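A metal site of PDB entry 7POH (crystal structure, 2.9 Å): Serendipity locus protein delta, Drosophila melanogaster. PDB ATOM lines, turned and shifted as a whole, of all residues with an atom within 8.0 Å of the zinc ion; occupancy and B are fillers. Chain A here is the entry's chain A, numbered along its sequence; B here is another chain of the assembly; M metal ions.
N of Arg 66 lies close to SG of Cys 64, at 3.7 Å.
The backbone NH (N) of Phe 9 lies close to the side-chain sulfur (SG) of Cys 7, at 3.4 Å.
SG of Cys 10 sits close to NH2 of Arg 66 (3.3 Å).
NH2 of Arg 66 lies close to SG of Cys 67 (3.5 Å).
The zinc ion is bound by SG of Cys 64 (2.3 Å), SG of Cys 7 (2.3 Å), SG of Cys 10 (2.3 Å) and SG of Cys 67 (2.3 Å).
Within 4 Å of the zinc ion: Cys 7, Cys 10, Cys 64 and Cys 67.
The nearest printed residue that does not touch the zinc ion is Phe 9 (4.1 Å).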
ATOM      1  N   THR A   6     -12.359  -2.186 -21.931  1.00  0.00           N
ATOM      2  CA  THR A   6     -13.746  -2.043 -21.366  1.00  0.00           C
ATOM      3  C   THR A   6     -13.740  -1.788 -19.846  1.00  0.00           C
ATOM      4  O   THR A   6     -13.297  -2.645 -19.081  1.00  0.00           O
ATOM      5  CB  THR A   6     -14.538  -3.329 -21.621  1.00  0.00           C
ATOM      6  OG1 THR A   6     -14.647  -3.396 -23.042  1.00  0.00           O
ATOM      7  CG2 THR A   6     -15.908  -3.334 -20.975  1.00  0.00           C
ATOM      8  N   CYS A   7     -14.300  -0.677 -19.408  1.00  0.00           N
ATOM      9  CA  CYS A   7     -14.331  -0.328 -17.964  1.00  0.00           C
ATOM     10  C   CYS A   7     -15.296  -1.254 -17.208  1.00  0.00           C
ATOM     11  O   CYS A   7     -16.508  -1.335 -17.574  1.00  0.00           O
ATOM     12  CB  CYS A   7     -14.745   1.110 -17.726  1.00  0.00           C
ATOM     13  SG  CYS A   7     -14.443   1.690 -16.115  1.00  0.00           S
ATOM     14  N   PHE A   8     -14.775  -1.857 -16.139  1.00  0.00           N
ATOM     15  CA  PHE A   8     -15.519  -2.695 -15.154  1.00  0.00           C
ATOM     16  C   PHE A   8     -16.560  -1.809 -14.431  1.00  0.00           C
ATOM     17  O   PHE A   8     -17.575  -2.301 -14.035  1.00  0.00           O
ATOM     18  CB  PHE A   8     -14.507  -3.515 -14.334  1.00  0.00           C
ATOM     19  CG  PHE A   8     -14.925  -3.749 -12.915  1.00  0.00           C
ATOM     20  CD1 PHE A   8     -14.911  -2.700 -12.007  1.00  0.00           C
ATOM     21  CD2 PHE A   8     -15.341  -5.009 -12.505  1.00  0.00           C
ATOM     22  CE1 PHE A   8     -15.365  -2.894 -10.709  1.00  0.00           C
ATOM     23  CE2 PHE A   8     -15.769  -5.216 -11.204  1.00  0.00           C
ATOM     24  CZ  PHE A   8     -15.786  -4.153 -10.311  1.00  0.00           C
ATOM     25  N   PHE A   9     -16.360  -0.493 -14.348  1.00  0.00           N
ATOM     26  CA  PHE A   9     -17.283   0.485 -13.739  1.00  0.00           C
ATOM     27  C   PHE A   9     -18.148   1.206 -14.834  1.00  0.00           C
ATOM     28  O   PHE A   9     -18.926   2.032 -14.386  1.00  0.00           O
ATOM     29  CB  PHE A   9     -16.323   1.357 -12.927  1.00  0.00           C
ATOM     30  CG  PHE A   9     -16.825   2.009 -11.647  1.00  0.00           C
ATOM     31  CD1 PHE A   9     -17.254   1.236 -10.570  1.00  0.00           C
ATOM     32  CD2 PHE A   9     -16.752   3.387 -11.456  1.00  0.00           C
ATOM     33  CE1 PHE A   9     -17.666   1.831  -9.396  1.00  0.00           C
ATOM     34  CE2 PHE A   9     -17.179   3.973 -10.269  1.00  0.00           C
ATOM     35  CZ  PHE A   9     -17.648   3.199  -9.252  1.00  0.00           C
ATOM     36  N   CYS A  10     -18.012   0.992 -16.196  1.00  0.00           N
ATOM     37  CA  CYS A  10     -18.939   1.426 -17.318  1.00  0.00           C
ATOM     38  C   CYS A  10     -18.598   0.857 -18.745  1.00  0.00           C
ATOM     39  O   CYS A  10     -19.147  -0.102 -19.041  1.00  0.00           O
ATOM     40  CB  CYS A  10     -19.143   2.941 -17.282  1.00  0.00           C
ATOM     41  SG  CYS A  10     -17.664   3.957 -16.979  1.00  0.00           S
ATOM     42  N   GLY A  11     -17.856   1.405 -19.738  1.00  0.00           N
ATOM     43  CA  GLY A  11     -17.764   0.817 -21.112  1.00  0.00           C
ATOM     44  C   GLY A  11     -16.559   1.328 -21.946  1.00  0.00           C
ATOM     45  O   GLY A  11     -15.708   1.963 -21.383  1.00  0.00           O
ATOM     46  N   ALA A  12     -16.636   1.201 -23.301  1.00  0.00           N
ATOM     47  CA  ALA A  12     -15.652   0.624 -24.267  1.00  0.00           C
ATOM     48  C   ALA A  12     -14.872   1.719 -25.029  1.00  0.00           C
ATOM     49  O   ALA A  12     -15.514   2.515 -25.673  1.00  0.00           O
ATOM     50  CB  ALA A  12     -16.374  -0.313 -25.251  1.00  0.00           C
ATOM     51  N   TYR A  26      -5.981   2.543 -19.837  1.00  0.00           N
ATOM     52  CA  TYR A  26      -6.873   1.917 -18.793  1.00  0.00           C
ATOM     53  C   TYR A  26      -6.037   1.193 -17.733  1.00  0.00           C
ATOM     54  O   TYR A  26      -5.083   0.494 -18.123  1.00  0.00           O
ATOM     55  CB  TYR A  26      -7.853   0.869 -19.356  1.00  0.00           C
ATOM     56  CG  TYR A  26      -9.124   1.373 -19.989  1.00  0.00           C
ATOM     57  CD1 TYR A  26      -9.141   2.545 -20.713  1.00  0.00           C
ATOM     58  CD2 TYR A  26     -10.304   0.658 -19.902  1.00  0.00           C
ATOM     59  CE1 TYR A  26     -10.298   3.012 -21.321  1.00  0.00           C
ATOM     60  CE2 TYR A  26     -11.471   1.102 -20.524  1.00  0.00           C
ATOM     61  CZ  TYR A  26     -11.475   2.288 -21.237  1.00  0.00           C
ATOM     62  OH  TYR A  26     -12.561   2.793 -21.873  1.00  0.00           O
ATOM     63  N   ARG A  62     -10.238  -3.978 -15.824  1.00  0.00           N
ATOM     64  CA  ARG A  62      -9.584  -2.673 -16.065  1.00  0.00           C
ATOM     65  C   ARG A  62     -10.549  -1.512 -15.747  1.00  0.00           C
ATOM     66  O   ARG A  62     -11.740  -1.766 -15.518  1.00  0.00           O
ATOM     67  CB  ARG A  62      -9.134  -2.594 -17.525  1.00  0.00           C
ATOM     68  CG  ARG A  62      -8.167  -3.689 -17.962  1.00  0.00           C
ATOM     69  CD  ARG A  62      -6.726  -3.308 -17.687  1.00  0.00           C
ATOM     70  NE  ARG A  62      -5.801  -4.422 -17.828  1.00  0.00           N
ATOM     71  CZ  ARG A  62      -5.682  -5.451 -16.974  1.00  0.00           C
ATOM     72  NH1 ARG A  62      -6.453  -5.542 -15.893  1.00  0.00           N
ATOM     73  NH2 ARG A  62      -4.779  -6.395 -17.200  1.00  0.00           N
ATOM     74  N   LEU A  63     -10.038  -0.279 -15.738  1.00  0.00           N
ATOM     75  CA  LEU A  63     -10.783   0.980 -15.439  1.00  0.00           C
ATOM     76  C   LEU A  63     -10.486   2.012 -16.521  1.00  0.00           C
ATOM     77  O   LEU A  63      -9.288   2.294 -16.760  1.00  0.00           O
ATOM     78  CB  LEU A  63     -10.331   1.548 -14.088  1.00  0.00           C
ATOM     79  CG  LEU A  63     -10.904   0.940 -12.812  1.00  0.00           C
ATOM     80  CD1 LEU A  63     -10.214   1.558 -11.607  1.00  0.00           C
ATOM     81  CD2 LEU A  63     -12.419   1.117 -12.698  1.00  0.00           C
ATOM     82  N   CYS A  64     -11.506   2.675 -17.057  1.00  0.00           N
ATOM     83  CA  CYS A  64     -11.289   3.885 -17.889  1.00  0.00           C
ATOM     84  C   CYS A  64     -10.446   4.860 -17.062  1.00  0.00           C
ATOM     85  O   CYS A  64     -10.380   4.791 -15.827  1.00  0.00           O
ATOM     86  CB  CYS A  64     -12.575   4.498 -18.413  1.00  0.00           C
ATOM     87  SG  CYS A  64     -13.717   5.171 -17.222  1.00  0.00           S
ATOM     88  N   PRO A  65      -9.745   5.819 -17.693  1.00  0.00           N
ATOM     89  CA  PRO A  65      -9.168   6.932 -16.925  1.00  0.00           C
ATOM     90  C   PRO A  65     -10.160   7.822 -16.138  1.00  0.00           C
ATOM     91  O   PRO A  65      -9.712   8.376 -15.158  1.00  0.00           O
ATOM     92  CB  PRO A  65      -8.446   7.712 -18.021  1.00  0.00           C
ATOM     93  CG  PRO A  65      -8.168   6.667 -19.065  1.00  0.00           C
ATOM     94  CD  PRO A  65      -9.456   5.889 -19.122  1.00  0.00           C
ATOM     95  N   ARG A  66     -11.422   7.954 -16.581  1.00  0.00           N
ATOM     96  CA  ARG A  66     -12.452   8.843 -15.978  1.00  0.00           C
ATOM     97  C   ARG A  66     -12.751   8.306 -14.576  1.00  0.00           C
ATOM     98  O   ARG A  66     -12.729   9.105 -13.598  1.00  0.00           O
ATOM     99  CB  ARG A  66     -13.738   8.894 -16.828  1.00  0.00           C
ATOM    100  CG  ARG A  66     -14.759   9.940 -16.418  1.00  0.00           C
ATOM    101  CD  ARG A  66     -16.118   9.888 -17.120  1.00  0.00           C
ATOM    102  NE  ARG A  66     -16.798   8.629 -16.926  1.00  0.00           N
ATOM    103  CZ  ARG A  66     -17.324   8.221 -15.777  1.00  0.00           C
ATOM    104  NH1 ARG A  66     -17.305   8.966 -14.686  1.00  0.00           N
ATOM    105  NH2 ARG A  66     -17.889   7.018 -15.691  1.00  0.00           N
ATOM    106  N   CYS A  67     -13.013   6.996 -14.531  1.00  0.00           N
ATOM    107  CA  CYS A  67     -13.406   6.217 -13.331  1.00  0.00           C
ATOM    108  C   CYS A  67     -12.215   6.210 -12.382  1.00  0.00           C
ATOM    109  O   CYS A  67     -12.384   6.601 -11.231  1.00  0.00           O
ATOM    110  CB  CYS A  67     -13.857   4.801 -13.691  1.00  0.00           C
ATOM    111  SG  CYS A  67     -15.393   4.868 -14.531  1.00  0.00           S
ATOM    112  N   PHE A  68     -11.036   5.875 -12.896  1.00  0.00           N
ATOM    113  CA  PHE A  68      -9.794   5.889 -12.069  1.00  0.00           C
ATOM    114  C   PHE A  68      -9.635   7.237 -11.338  1.00  0.00           C
ATOM    115  O   PHE A  68      -9.226   7.249 -10.153  1.00  0.00           O
ATOM    116  CB  PHE A  68      -8.550   5.577 -12.902  1.00  0.00           C
ATOM    117  CG  PHE A  68      -7.331   5.467 -12.021  1.00  0.00           C
ATOM    118  CD1 PHE A  68      -7.203   4.399 -11.135  1.00  0.00           C
ATOM    119  CD2 PHE A  68      -6.379   6.469 -11.999  1.00  0.00           C
ATOM    120  CE1 PHE A  68      -6.119   4.329 -10.285  1.00  0.00           C
ATOM    121  CE2 PHE A  68      -5.309   6.389 -11.135  1.00  0.00           C
ATOM    122  CZ  PHE A  68      -5.165   5.314 -10.281  1.00  0.00           C
ATOM    123  N   GLU A  70     -12.236   9.498 -10.701  1.00  0.00           N
ATOM    124  CA  GLU A  70     -13.385   9.519  -9.762  1.00  0.00           C
ATOM    125  C   GLU A  70     -12.979   8.868  -8.445  1.00  0.00           C
ATOM    126  O   GLU A  70     -13.346   9.444  -7.377  1.00  0.00           O
ATOM    127  CB  GLU A  70     -14.552   8.669 -10.273  1.00  0.00           C
ATOM    128  CG  GLU A  70     -15.445   9.292 -11.294  1.00  0.00           C
ATOM    129  CD  GLU A  70     -16.329  10.392 -10.746  1.00  0.00           C
ATOM    130  OE1 GLU A  70     -15.726  11.431 -10.204  1.00  0.00           O
ATOM    131  OE2 GLU A  70     -17.612  10.227 -10.910  1.00  0.00           O
ATOM    132  N   GLN B  91     -23.353   4.230  -8.858  1.00  0.00           N
ATOM    133  CA  GLN B  91     -22.647   3.720 -10.054  1.00  0.00           C
ATOM    134  C   GLN B  91     -22.484   2.211  -9.886  1.00  0.00           C
ATOM    135  O   GLN B  91     -22.873   1.477 -10.806  1.00  0.00           O
ATOM    136  CB  GLN B  91     -21.299   4.447 -10.213  1.00  0.00           C
ATOM    137  CG  GLN B  91     -20.537   4.086 -11.498  1.00  0.00           C
ATOM    138  CD  GLN B  91     -21.294   4.619 -12.678  1.00  0.00           C
ATOM    139  OE1 GLN B  91     -21.506   5.817 -12.765  1.00  0.00           O
ATOM    140  NE2 GLN B  91     -21.783   3.727 -13.505  1.00  0.00           N
HETATM  141 ZN    ZN M   1     -15.388   3.752 -16.576  1.00  0.00          ZN
